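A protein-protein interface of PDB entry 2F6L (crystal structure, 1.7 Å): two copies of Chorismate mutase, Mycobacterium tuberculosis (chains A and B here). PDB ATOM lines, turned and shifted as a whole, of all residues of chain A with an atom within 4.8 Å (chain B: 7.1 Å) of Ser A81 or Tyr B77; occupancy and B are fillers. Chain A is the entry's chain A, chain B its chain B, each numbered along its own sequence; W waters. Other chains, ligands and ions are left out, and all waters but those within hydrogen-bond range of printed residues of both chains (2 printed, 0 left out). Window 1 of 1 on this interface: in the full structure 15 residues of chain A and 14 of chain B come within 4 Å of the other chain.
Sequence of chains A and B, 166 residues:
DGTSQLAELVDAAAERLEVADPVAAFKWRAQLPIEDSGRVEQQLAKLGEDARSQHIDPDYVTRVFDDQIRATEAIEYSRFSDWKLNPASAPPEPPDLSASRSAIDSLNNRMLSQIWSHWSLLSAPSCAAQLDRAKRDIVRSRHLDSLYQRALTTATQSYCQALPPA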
ATOM      1  N   TYR A  77      24.680 -20.295  10.927  1.00  0.00           N
ATOM      2  CA  TYR A  77      23.830 -19.813  12.040  1.00  0.00           C
ATOM      3  C   TYR A  77      22.475 -19.300  11.559  1.00  0.00           C
ATOM      4  O   TYR A  77      21.478 -19.496  12.273  1.00  0.00           O
ATOM      5  CB  TYR A  77      24.535 -18.666  12.754  1.00  0.00           C
ATOM      6  CG  TYR A  77      25.522 -19.084  13.830  1.00  0.00           C
ATOM      7  CD1 TYR A  77      25.145 -19.938  14.897  1.00  0.00           C
ATOM      8  CD2 TYR A  77      26.839 -18.599  13.831  1.00  0.00           C
ATOM      9  CE1 TYR A  77      26.069 -20.304  15.928  1.00  0.00           C
ATOM     10  CE2 TYR A  77      27.738 -18.966  14.857  1.00  0.00           C
ATOM     11  CZ  TYR A  77      27.354 -19.810  15.879  1.00  0.00           C
ATOM     12  OH  TYR A  77      28.239 -20.160  16.906  1.00  0.00           O
ATOM     13  N   SER A  78      22.418 -18.667  10.376  1.00  0.00           N
ATOM     14  CA  SER A  78      21.123 -18.154   9.822  1.00  0.00           C
ATOM     15  C   SER A  78      20.185 -19.322   9.535  1.00  0.00           C
ATOM     16  O   SER A  78      18.997 -19.283   9.848  1.00  0.00           O
ATOM     17  CB  SER A  78      21.357 -17.339   8.546  1.00  0.00           C
ATOM     18  OG  SER A  78      20.140 -16.768   8.075  1.00  0.00           O
ATOM     19  N   ARG A  79      20.761 -20.396   8.986  1.00  0.00           N
ATOM     20  CA  ARG A  79      19.974 -21.620   8.753  1.00  0.00           C
ATOM     21  C   ARG A  79      19.478 -22.174  10.073  1.00  0.00           C
ATOM     22  O   ARG A  79      18.286 -22.544  10.176  1.00  0.00           O
ATOM     23  CB  ARG A  79      20.816 -22.680   8.019  1.00  0.00           C
ATOM     24  CG  ARG A  79      21.295 -22.328   6.603  1.00  0.00           C
ATOM     25  CD  ARG A  79      20.322 -21.543   5.786  1.00  0.00           C
ATOM     26  NE  ARG A  79      20.752 -21.448   4.351  1.00  0.00           N
ATOM     27  CZ  ARG A  79      20.423 -20.464   3.518  1.00  0.00           C
ATOM     28  NH1 ARG A  79      19.684 -19.425   3.933  1.00  0.00           N
ATOM     29  NH2 ARG A  79      20.815 -20.521   2.228  1.00  0.00           N
ATOM     30  N   PHE A  80      20.367 -22.321  11.074  1.00  0.00           N
ATOM     31  CA  PHE A  80      19.941 -22.827  12.391  1.00  0.00           C
ATOM     32  C   PHE A  80      18.797 -21.984  12.939  1.00  0.00           C
ATOM     33  O   PHE A  80      17.849 -22.523  13.493  1.00  0.00           O
ATOM     34  CB  PHE A  80      21.083 -22.856  13.398  1.00  0.00           C
ATOM     35  CG  PHE A  80      21.870 -24.154  13.392  1.00  0.00           C
ATOM     36  CD1 PHE A  80      22.055 -24.868  12.191  1.00  0.00           C
ATOM     37  CD2 PHE A  80      22.400 -24.652  14.595  1.00  0.00           C
ATOM     38  CE1 PHE A  80      22.820 -26.093  12.202  1.00  0.00           C
ATOM     39  CE2 PHE A  80      23.146 -25.860  14.632  1.00  0.00           C
ATOM     40  CZ  PHE A  80      23.362 -26.565  13.414  1.00  0.00           C
ATOM     41  N   SER A  81      18.850 -20.660  12.729  1.00  0.00           N
ATOM     42  CA  SER A  81      17.747 -19.783  13.194  1.00  0.00           C
ATOM     43  C   SER A  81      16.428 -20.151  12.516  1.00  0.00           C
ATOM     44  O   SER A  81      15.377 -20.281  13.169  1.00  0.00           O
ATOM     45  CB  SER A  81      18.102 -18.293  12.932  1.00  0.00           C
ATOM     46  OG  SER A  81      17.018 -17.417  13.305  1.00  0.00           O
ATOM     47  N   ASP A  82      16.463 -20.291  11.196  1.00  0.00           N
ATOM     48  CA  ASP A  82      15.296 -20.704  10.400  1.00  0.00           C
ATOM     49  C   ASP A  82      14.744 -22.045  10.852  1.00  0.00           C
ATOM     50  O   ASP A  82      13.533 -22.207  11.034  1.00  0.00           O
ATOM     51  CB  ASP A  82      15.692 -20.820   8.940  1.00  0.00           C
ATOM     52  CG  ASP A  82      16.005 -19.465   8.277  1.00  0.00           C
ATOM     53  OD1 ASP A  82      15.691 -18.381   8.821  1.00  0.00           O
ATOM     54  OD2 ASP A  82      16.634 -19.542   7.180  1.00  0.00           O
ATOM     55  N   TRP A  83      15.630 -23.024  11.038  1.00  0.00           N
ATOM     56  CA  TRP A  83      15.202 -24.386  11.362  1.00  0.00           C
ATOM     57  C   TRP A  83      14.676 -24.500  12.793  1.00  0.00           C
ATOM     58  O   TRP A  83      13.831 -25.356  13.103  1.00  0.00           O
ATOM     59  CB  TRP A  83      16.355 -25.363  11.104  1.00  0.00           C
ATOM     60  CG  TRP A  83      16.769 -25.351   9.634  1.00  0.00           C
ATOM     61  CD1 TRP A  83      16.002 -24.967   8.554  1.00  0.00           C
ATOM     62  CD2 TRP A  83      18.062 -25.712   9.087  1.00  0.00           C
ATOM     63  NE1 TRP A  83      16.727 -25.088   7.382  1.00  0.00           N
ATOM     64  CE2 TRP A  83      17.986 -25.546   7.680  1.00  0.00           C
ATOM     65  CE3 TRP A  83      19.258 -26.167   9.652  1.00  0.00           C
ATOM     66  CZ2 TRP A  83      19.100 -25.797   6.805  1.00  0.00           C
ATOM     67  CZ3 TRP A  83      20.363 -26.431   8.775  1.00  0.00           C
ATOM     68  CH2 TRP A  83      20.251 -26.254   7.388  1.00  0.00           C
ATOM     69  N   LYS A  84      15.163 -23.629  13.661  1.00  0.00           N
ATOM     70  CA  LYS A  84      14.612 -23.567  14.996  1.00  0.00           C
ATOM     71  C   LYS A  84      13.175 -23.085  14.965  1.00  0.00           C
ATOM     72  O   LYS A  84      12.339 -23.618  15.678  1.00  0.00           O
ATOM     73  CB  LYS A  84      15.480 -22.683  15.893  1.00  0.00           C
ATOM     74  CG  LYS A  84      15.056 -22.661  17.356  1.00  0.00           C
ATOM     75  CD  LYS A  84      15.257 -24.002  18.071  1.00  0.00           C
ATOM     76  CE  LYS A  84      16.672 -24.247  18.464  1.00  0.00           C
ATOM     77  NZ  LYS A  84      16.785 -25.265  19.613  1.00  0.00           N
ATOM     78  N   LEU A  85      12.858 -22.087  14.139  1.00  0.00           N
ATOM     79  CA  LEU A  85      11.465 -21.651  14.031  1.00  0.00           C
ATOM     80  C   LEU A  85      10.573 -22.714  13.348  1.00  0.00           C
ATOM     81  O   LEU A  85       9.452 -23.032  13.821  1.00  0.00           O
ATOM     82  CB  LEU A  85      11.389 -20.313  13.296  1.00  0.00           C
ATOM     83  CG  LEU A  85      12.111 -19.158  14.008  1.00  0.00           C
ATOM     84  CD1 LEU A  85      12.085 -17.963  13.098  1.00  0.00           C
ATOM     85  CD2 LEU A  85      11.447 -18.852  15.382  1.00  0.00           C
ATOM     86  N   ALA B  24      22.071 -13.422  24.136  1.00  0.00           N
ATOM     87  CA  ALA B  24      23.012 -13.754  23.042  1.00  0.00           C
ATOM     88  C   ALA B  24      24.320 -12.982  23.190  1.00  0.00           C
ATOM     89  O   ALA B  24      25.396 -13.571  23.080  1.00  0.00           O
ATOM     90  CB  ALA B  24      22.385 -13.442  21.683  1.00  0.00           C
ATOM     91  N   PRO B  33      27.843 -21.783  24.501  1.00  0.00           N
ATOM     92  CA  PRO B  33      26.888 -22.310  23.522  1.00  0.00           C
ATOM     93  C   PRO B  33      25.467 -21.750  23.641  1.00  0.00           C
ATOM     94  O   PRO B  33      24.991 -21.482  24.758  1.00  0.00           O
ATOM     95  CB  PRO B  33      26.884 -23.807  23.808  1.00  0.00           C
ATOM     96  CG  PRO B  33      27.362 -23.925  25.244  1.00  0.00           C
ATOM     97  CD  PRO B  33      28.382 -22.834  25.382  1.00  0.00           C
ATOM     98  N   ILE B  34      24.788 -21.601  22.498  1.00  0.00           N
ATOM     99  CA  ILE B  34      23.382 -21.173  22.487  1.00  0.00           C
ATOM    100  C   ILE B  34      22.498 -22.249  23.089  1.00  0.00           C
ATOM    101  O   ILE B  34      21.703 -21.943  23.990  1.00  0.00           O
ATOM    102  CB  ILE B  34      22.896 -20.740  21.076  1.00  0.00           C
ATOM    103  CG1 ILE B  34      23.539 -19.401  20.691  1.00  0.00           C
ATOM    104  CG2 ILE B  34      21.363 -20.597  21.032  1.00  0.00           C
ATOM    105  CD1 ILE B  34      23.423 -19.031  19.245  1.00  0.00           C
ATOM    106  N   GLU B  35      22.671 -23.503  22.654  1.00  0.00           N
ATOM    107  CA  GLU B  35      21.868 -24.626  23.189  1.00  0.00           C
ATOM    108  C   GLU B  35      22.207 -24.983  24.646  1.00  0.00           C
ATOM    109  O   GLU B  35      23.320 -24.726  25.135  1.00  0.00           O
ATOM    110  CB  GLU B  35      21.998 -25.890  22.335  1.00  0.00           C
ATOM    111  CG  GLU B  35      21.615 -25.756  20.857  1.00  0.00           C
ATOM    112  CD  GLU B  35      20.110 -25.824  20.614  1.00  0.00           C
ATOM    113  OE1 GLU B  35      19.415 -26.466  21.416  1.00  0.00           O
ATOM    114  OE2 GLU B  35      19.622 -25.270  19.595  1.00  0.00           O
ATOM    115  N   ARG B  70      11.945 -21.924  22.183  1.00  0.00           N
ATOM    116  CA  ARG B  70      12.388 -22.168  20.794  1.00  0.00           C
ATOM    117  C   ARG B  70      12.596 -20.832  20.039  1.00  0.00           C
ATOM    118  O   ARG B  70      13.620 -20.597  19.399  1.00  0.00           O
ATOM    119  CB  ARG B  70      11.320 -23.046  20.099  1.00  0.00           C
ATOM    120  CG  ARG B  70      11.527 -23.303  18.608  1.00  0.00           C
ATOM    121  CD  ARG B  70      10.300 -24.084  17.989  1.00  0.00           C
ATOM    122  NE  ARG B  70      10.263 -25.453  18.477  1.00  0.00           N
ATOM    123  CZ  ARG B  70      11.084 -26.421  18.040  1.00  0.00           C
ATOM    124  NH1 ARG B  70      11.984 -26.150  17.099  1.00  0.00           N
ATOM    125  NH2 ARG B  70      11.017 -27.662  18.538  1.00  0.00           N
ATOM    126  N   ALA B  71      11.635 -19.930  20.142  1.00  0.00           N
ATOM    127  CA  ALA B  71      11.712 -18.694  19.391  1.00  0.00           C
ATOM    128  C   ALA B  71      12.893 -17.857  19.898  1.00  0.00           C
ATOM    129  O   ALA B  71      13.538 -17.134  19.121  1.00  0.00           O
ATOM    130  CB  ALA B  71      10.411 -17.920  19.564  1.00  0.00           C
ATOM    131  N   THR B  72      13.142 -17.930  21.207  1.00  0.00           N
ATOM    132  CA  THR B  72      14.224 -17.116  21.838  1.00  0.00           C
ATOM    133  C   THR B  72      15.569 -17.653  21.264  1.00  0.00           C
ATOM    134  O   THR B  72      16.400 -16.883  20.854  1.00  0.00           O
ATOM    135  CB  THR B  72      14.167 -17.313  23.356  1.00  0.00           C
ATOM    136  OG1 THR B  72      12.845 -16.949  23.840  1.00  0.00           O
ATOM    137  CG2 THR B  72      15.223 -16.472  24.085  1.00  0.00           C
ATOM    138  N   GLU B  73      15.732 -18.971  21.250  1.00  0.00           N
ATOM    139  CA  GLU B  73      16.933 -19.593  20.650  1.00  0.00           C
ATOM    140  C   GLU B  73      17.105 -19.204  19.194  1.00  0.00           C
ATOM    141  O   GLU B  73      18.240 -18.936  18.749  1.00  0.00           O
ATOM    142  CB  GLU B  73      16.897 -21.107  20.843  1.00  0.00           C
ATOM    143  CG  GLU B  73      16.941 -21.502  22.330  1.00  0.00           C
ATOM    144  CD  GLU B  73      16.766 -22.976  22.556  1.00  0.00           C
ATOM    145  OE1 GLU B  73      16.093 -23.642  21.761  1.00  0.00           O
ATOM    146  OE2 GLU B  73      17.325 -23.471  23.558  1.00  0.00           O
ATOM    147  N   ALA B  74      15.994 -19.155  18.435  1.00  0.00           N
ATOM    148  CA  ALA B  74      16.093 -18.751  17.051  1.00  0.00           C
ATOM    149  C   ALA B  74      16.675 -17.332  16.912  1.00  0.00           C
ATOM    150  O   ALA B  74      17.479 -17.036  16.007  1.00  0.00           O
ATOM    151  CB  ALA B  74      14.691 -18.860  16.344  1.00  0.00           C
ATOM    152  N   ILE B  75      16.250 -16.429  17.783  1.00  0.00           N
ATOM    153  CA  ILE B  75      16.786 -15.061  17.782  1.00  0.00           C
ATOM    154  C   ILE B  75      18.297 -15.053  18.108  1.00  0.00           C
ATOM    155  O   ILE B  75      19.070 -14.360  17.428  1.00  0.00           O
ATOM    156  CB  ILE B  75      15.974 -14.122  18.710  1.00  0.00           C
ATOM    157  CG1 ILE B  75      14.539 -13.930  18.152  1.00  0.00           C
ATOM    158  CG2 ILE B  75      16.745 -12.739  18.898  1.00  0.00           C
ATOM    159  CD1 ILE B  75      13.524 -13.313  19.239  1.00  0.00           C
ATOM    160  N   GLU B  76      18.705 -15.836  19.111  1.00  0.00           N
ATOM    161  CA  GLU B  76      20.118 -15.894  19.529  1.00  0.00           C
ATOM    162  C   GLU B  76      20.945 -16.368  18.324  1.00  0.00           C
ATOM    163  O   GLU B  76      21.955 -15.749  17.991  1.00  0.00           O
ATOM    164  CB  GLU B  76      20.290 -16.836  20.705  1.00  0.00           C
ATOM    165  CG  GLU B  76      19.553 -16.345  21.982  1.00  0.00           C
ATOM    166  CD  GLU B  76      19.646 -17.347  23.110  1.00  0.00           C
ATOM    167  OE1 GLU B  76      20.769 -17.746  23.482  1.00  0.00           O
ATOM    168  OE2 GLU B  76      18.566 -17.743  23.617  1.00  0.00           O
ATOM    169  N   TYR B  77      20.453 -17.376  17.612  1.00  0.00           N
ATOM    170  CA  TYR B  77      21.153 -17.832  16.364  1.00  0.00           C
ATOM    171  C   TYR B  77      21.281 -16.749  15.312  1.00  0.00           C
ATOM    172  O   TYR B  77      22.365 -16.592  14.706  1.00  0.00           O
ATOM    173  CB  TYR B  77      20.471 -19.059  15.740  1.00  0.00           C
ATOM    174  CG  TYR B  77      20.761 -20.377  16.442  1.00  0.00           C
ATOM    175  CD1 TYR B  77      22.059 -20.802  16.703  1.00  0.00           C
ATOM    176  CD2 TYR B  77      19.717 -21.223  16.779  1.00  0.00           C
ATOM    177  CE1 TYR B  77      22.318 -22.049  17.333  1.00  0.00           C
ATOM    178  CE2 TYR B  77      19.959 -22.477  17.359  1.00  0.00           C
ATOM    179  CZ  TYR B  77      21.245 -22.864  17.671  1.00  0.00           C
ATOM    180  OH  TYR B  77      21.438 -24.109  18.264  1.00  0.00           O
ATOM    181  N   SER B  78      20.197 -16.008  15.080  1.00  0.00           N
ATOM    182  CA  SER B  78      20.218 -14.935  14.090  1.00  0.00           C
ATOM    183  C   SER B  78      21.206 -13.859  14.523  1.00  0.00           C
ATOM    184  O   SER B  78      21.942 -13.316  13.679  1.00  0.00           O
ATOM    185  CB  SER B  78      18.835 -14.342  13.976  1.00  0.00           C
ATOM    186  OG  SER B  78      18.785 -13.430  12.909  1.00  0.00           O
ATOM    187  N   ARG B  79      21.232 -13.528  15.824  1.00  0.00           N
ATOM    188  CA  ARG B  79      22.216 -12.499  16.255  1.00  0.00           C
ATOM    189  C   ARG B  79      23.654 -13.005  16.036  1.00  0.00           C
ATOM    190  O   ARG B  79      24.530 -12.245  15.591  1.00  0.00           O
ATOM    191  CB  ARG B  79      22.030 -12.148  17.723  1.00  0.00           C
ATOM    192  CG  ARG B  79      20.684 -11.416  17.994  1.00  0.00           C
ATOM    193  CD  ARG B  79      20.558 -10.243  17.113  1.00  0.00           C
ATOM    194  NE  ARG B  79      19.631  -9.273  17.692  1.00  0.00           N
ATOM    195  CZ  ARG B  79      18.569  -8.782  17.055  1.00  0.00           C
ATOM    196  NH1 ARG B  79      18.323  -9.160  15.801  1.00  0.00           N
ATOM    197  NH2 ARG B  79      17.781  -7.874  17.665  1.00  0.00           N
ATOM    198  N   PHE B  80      23.914 -14.271  16.376  1.00  0.00           N
ATOM    199  CA  PHE B  80      25.275 -14.812  16.123  1.00  0.00           C
ATOM    200  C   PHE B  80      25.630 -14.736  14.647  1.00  0.00           C
ATOM    201  O   PHE B  80      26.795 -14.469  14.294  1.00  0.00           O
ATOM    202  CB  PHE B  80      25.427 -16.247  16.627  1.00  0.00           C
ATOM    203  CG  PHE B  80      25.802 -16.347  18.097  1.00  0.00           C
ATOM    204  CD1 PHE B  80      25.229 -15.501  19.053  1.00  0.00           C
ATOM    205  CD2 PHE B  80      26.722 -17.299  18.508  1.00  0.00           C
ATOM    206  CE1 PHE B  80      25.607 -15.636  20.415  1.00  0.00           C
ATOM    207  CE2 PHE B  80      27.100 -17.440  19.828  1.00  0.00           C
ATOM    208  CZ  PHE B  80      26.531 -16.613  20.787  1.00  0.00           C
ATOM    209  N   SER B  81      24.680 -15.003  13.764  1.00  0.00           N
ATOM    210  CA  SER B  81      24.939 -14.837  12.312  1.00  0.00           C
ATOM    211  C   SER B  81      25.375 -13.380  12.053  1.00  0.00           C
ATOM    212  O   SER B  81      26.351 -13.123  11.366  1.00  0.00           O
ATOM    213  CB  SER B  81      23.638 -15.079  11.542  1.00  0.00           C
ATOM    214  OG  SER B  81      23.835 -14.936  10.173  1.00  0.00           O
ATOM    215  N   ASP B  82      24.592 -12.423  12.572  1.00  0.00           N
ATOM    216  CA  ASP B  82      24.892 -10.994  12.341  1.00  0.00           C
ATOM    217  C   ASP B  82      26.273 -10.612  12.839  1.00  0.00           C
ATOM    218  O   ASP B  82      26.995  -9.836  12.176  1.00  0.00           O
ATOM    219  CB  ASP B  82      23.846 -10.107  13.026  1.00  0.00           C
ATOM    220  CG  ASP B  82      22.449 -10.147  12.345  1.00  0.00           C
ATOM    221  OD1 ASP B  82      22.256 -10.580  11.185  1.00  0.00           O
ATOM    222  OD2 ASP B  82      21.507  -9.715  13.055  1.00  0.00           O
ATOM    223  N   TRP B  83      26.638 -11.149  14.003  1.00  0.00           N
ATOM    224  CA  TRP B  83      27.888 -10.783  14.656  1.00  0.00           C
ATOM    225  C   TRP B  83      29.096 -11.471  14.013  1.00  0.00           C
ATOM    226  O   TRP B  83      30.208 -10.927  14.075  1.00  0.00           O
ATOM    227  CB  TRP B  83      27.793 -11.047  16.137  1.00  0.00           C
ATOM    228  CG  TRP B  83      26.680 -10.227  16.769  1.00  0.00           C
ATOM    229  CD1 TRP B  83      26.164  -9.045  16.323  1.00  0.00           C
ATOM    230  CD2 TRP B  83      25.986 -10.536  17.996  1.00  0.00           C
ATOM    231  NE1 TRP B  83      25.146  -8.592  17.194  1.00  0.00           N
ATOM    232  CE2 TRP B  83      25.024  -9.500  18.213  1.00  0.00           C
ATOM    233  CE3 TRP B  83      26.053 -11.601  18.901  1.00  0.00           C
ATOM    234  CZ2 TRP B  83      24.159  -9.496  19.322  1.00  0.00           C
ATOM    235  CZ3 TRP B  83      25.170 -11.585  20.020  1.00  0.00           C
ATOM    236  CH2 TRP B  83      24.259 -10.528  20.201  1.00  0.00           C
ATOM    237  N   LEU B 147      12.550 -10.670  11.612  1.00  0.00           N
ATOM    238  CA  LEU B 147      12.940 -11.755  12.543  1.00  0.00           C
ATOM    239  C   LEU B 147      11.993 -11.874  13.764  1.00  0.00           C
ATOM    240  O   LEU B 147      11.497 -12.970  14.084  1.00  0.00           O
ATOM    241  CB  LEU B 147      14.394 -11.601  13.028  1.00  0.00           C
ATOM    242  CG  LEU B 147      14.910 -12.504  14.179  1.00  0.00           C
ATOM    243  CD1 LEU B 147      14.947 -13.964  13.807  1.00  0.00           C
ATOM    244  CD2 LEU B 147      16.216 -12.056  14.685  1.00  0.00           C
ATOM    245  N   ARG B 150       8.504 -13.216  12.821  1.00  0.00           N
ATOM    246  CA  ARG B 150       8.493 -14.689  12.706  1.00  0.00           C
ATOM    247  C   ARG B 150       8.586 -15.373  14.075  1.00  0.00           C
ATOM    248  O   ARG B 150       7.903 -16.385  14.327  1.00  0.00           O
ATOM    249  CB  ARG B 150       9.649 -15.151  11.786  1.00  0.00           C
ATOM    250  CG  ARG B 150       9.444 -14.613  10.343  1.00  0.00           C
ATOM    251  CD  ARG B 150      10.798 -14.612   9.546  1.00  0.00           C
ATOM    252  NE  ARG B 150      11.294 -15.979   9.479  1.00  0.00           N
ATOM    253  CZ  ARG B 150      12.572 -16.328   9.649  1.00  0.00           C
ATOM    254  NH1 ARG B 150      13.489 -15.386   9.910  1.00  0.00           N
ATOM    255  NH2 ARG B 150      12.920 -17.624   9.561  1.00  0.00           N
HETATM  256  O   HOH W   1      11.887 -20.530   9.617  1.00  0.00           O
HETATM  257  O   HOH W   2      16.109 -16.508  10.875  1.00  0.00           O
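OG of Ser A81 lies within hydrogen-bond range of O of Ala B74 (2.8 Å).
The guanidinium group (NH2) of Arg B150 is in salt-bridge range of the side-chain carboxylate (OD1) of Asp A82.
NZ of Lys A84 is in salt-bridge range of OE2 of Glu B35 (2.8 Å).
The backbone carbonyl oxygen of Lys A84 is in hydrogen-bond range of the guanidinium group of Arg B70, at 2.9 Å.
The side-chain amino group of Lys A84 is in salt-bridge range of the side-chain carboxylate of Glu B73 (2.8 Å).
The side-chain carboxylate (OE2) of Glu B35 sits at hydrogen-bond distance from the side-chain hydroxyl (OH) of Tyr B77 (2.5 Å).
Among the printed residues, merely in contact across the chains: Leu A85 with Ala B74 (3.4 Å), Tyr A77 with Tyr B77 (3.6 Å), Tyr A77 with Phe B80 (3.6 Å), Ser A81 with Ser B78 (3.6 Å), Leu A85 with Arg B150 (3.7 Å), Phe A80 with Tyr B77 (3.7 Å), Ser A81 with Tyr B77 (3.8 Å), Lys A84 with Ala B74 (3.8 Å), Tyr A77 with Ser B81 (3.8 Å), Ser A78 with Ser B81 (3.8 Å) and Lys A84 with Tyr B77 (3.9 Å).
Of chain A, only Tyr A77, Phe A80, Ser A81 and Lys A84 come within 4 Å of Tyr B77.
Of the printed residues of chain B, Asp A82 touches Arg B150.
Of the printed residues of chain A, Ser B81 touches Tyr A77 and Ser A78.
Trp B83 touches none of the printed residues of chain A.
Ile B34 touches none of the printed residues of chain A.
The nearest residue of chain B that does not touch Ser A81 is Leu B147 (4.1 Å).
The nearest printed residue of chain A that does not touch Tyr B77 is Ser A78 (4.8 Å).
The nearest printed residue of chain B that does not touch Lys A84 is Ala B71 (5.2 Å).
Printed residues of chain B that touch a printed residue of chain A: Glu B35, Arg B70, Glu B73, Ala B74, Tyr B77, Ser B78, Phe B80, Ser B81 and Arg B150.
Hydrophobic or aromatic side chains of chain B within 4 Å of the printed part of chain A: Ala B74, Tyr B77 and Phe B80.
Hydrophobic or aromatic side chains of chain A within 4 Å of the printed part of chain B: Tyr A77, Phe A80 and Leu A85.
Along chain A the printed residues that touch a printed residue of chain B span positions 77 to 85.
Among the printed residues, 16 pairs touch across the chains.
Tyr B77 touches its own counterpart, Tyr A77.
Tyr A77 touches Phe B80, and with the chains exchanged Phe A80 touches Tyr B77.
Tyr A77 touches Ser B81, and with the chains exchanged Ser A81 touches Tyr B77.
Ser A78 touches Ser B81, and with the chains exchanged Ser A81 touches Ser B78.
Positions printed for both chains: 77, 78, 79, 80, 81, 82 and 83.
Of the 16 pairs that touch across the chains among the printed residues, 7 have their exchanged pair printed and touching as well.
Water W1 lies within hydrogen-bond range of the backbone carbonyl oxygen of Asp A82 (2.7 Å) and the guanidinium group of Arg B150 (3.1 Å).
Water W2 lies within hydrogen-bond range of the side-chain hydroxyl (OG) of Ser A81, the side-chain carboxylate (OD1) of Asp A82 and the guanidinium group (NH1) of Arg B150.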
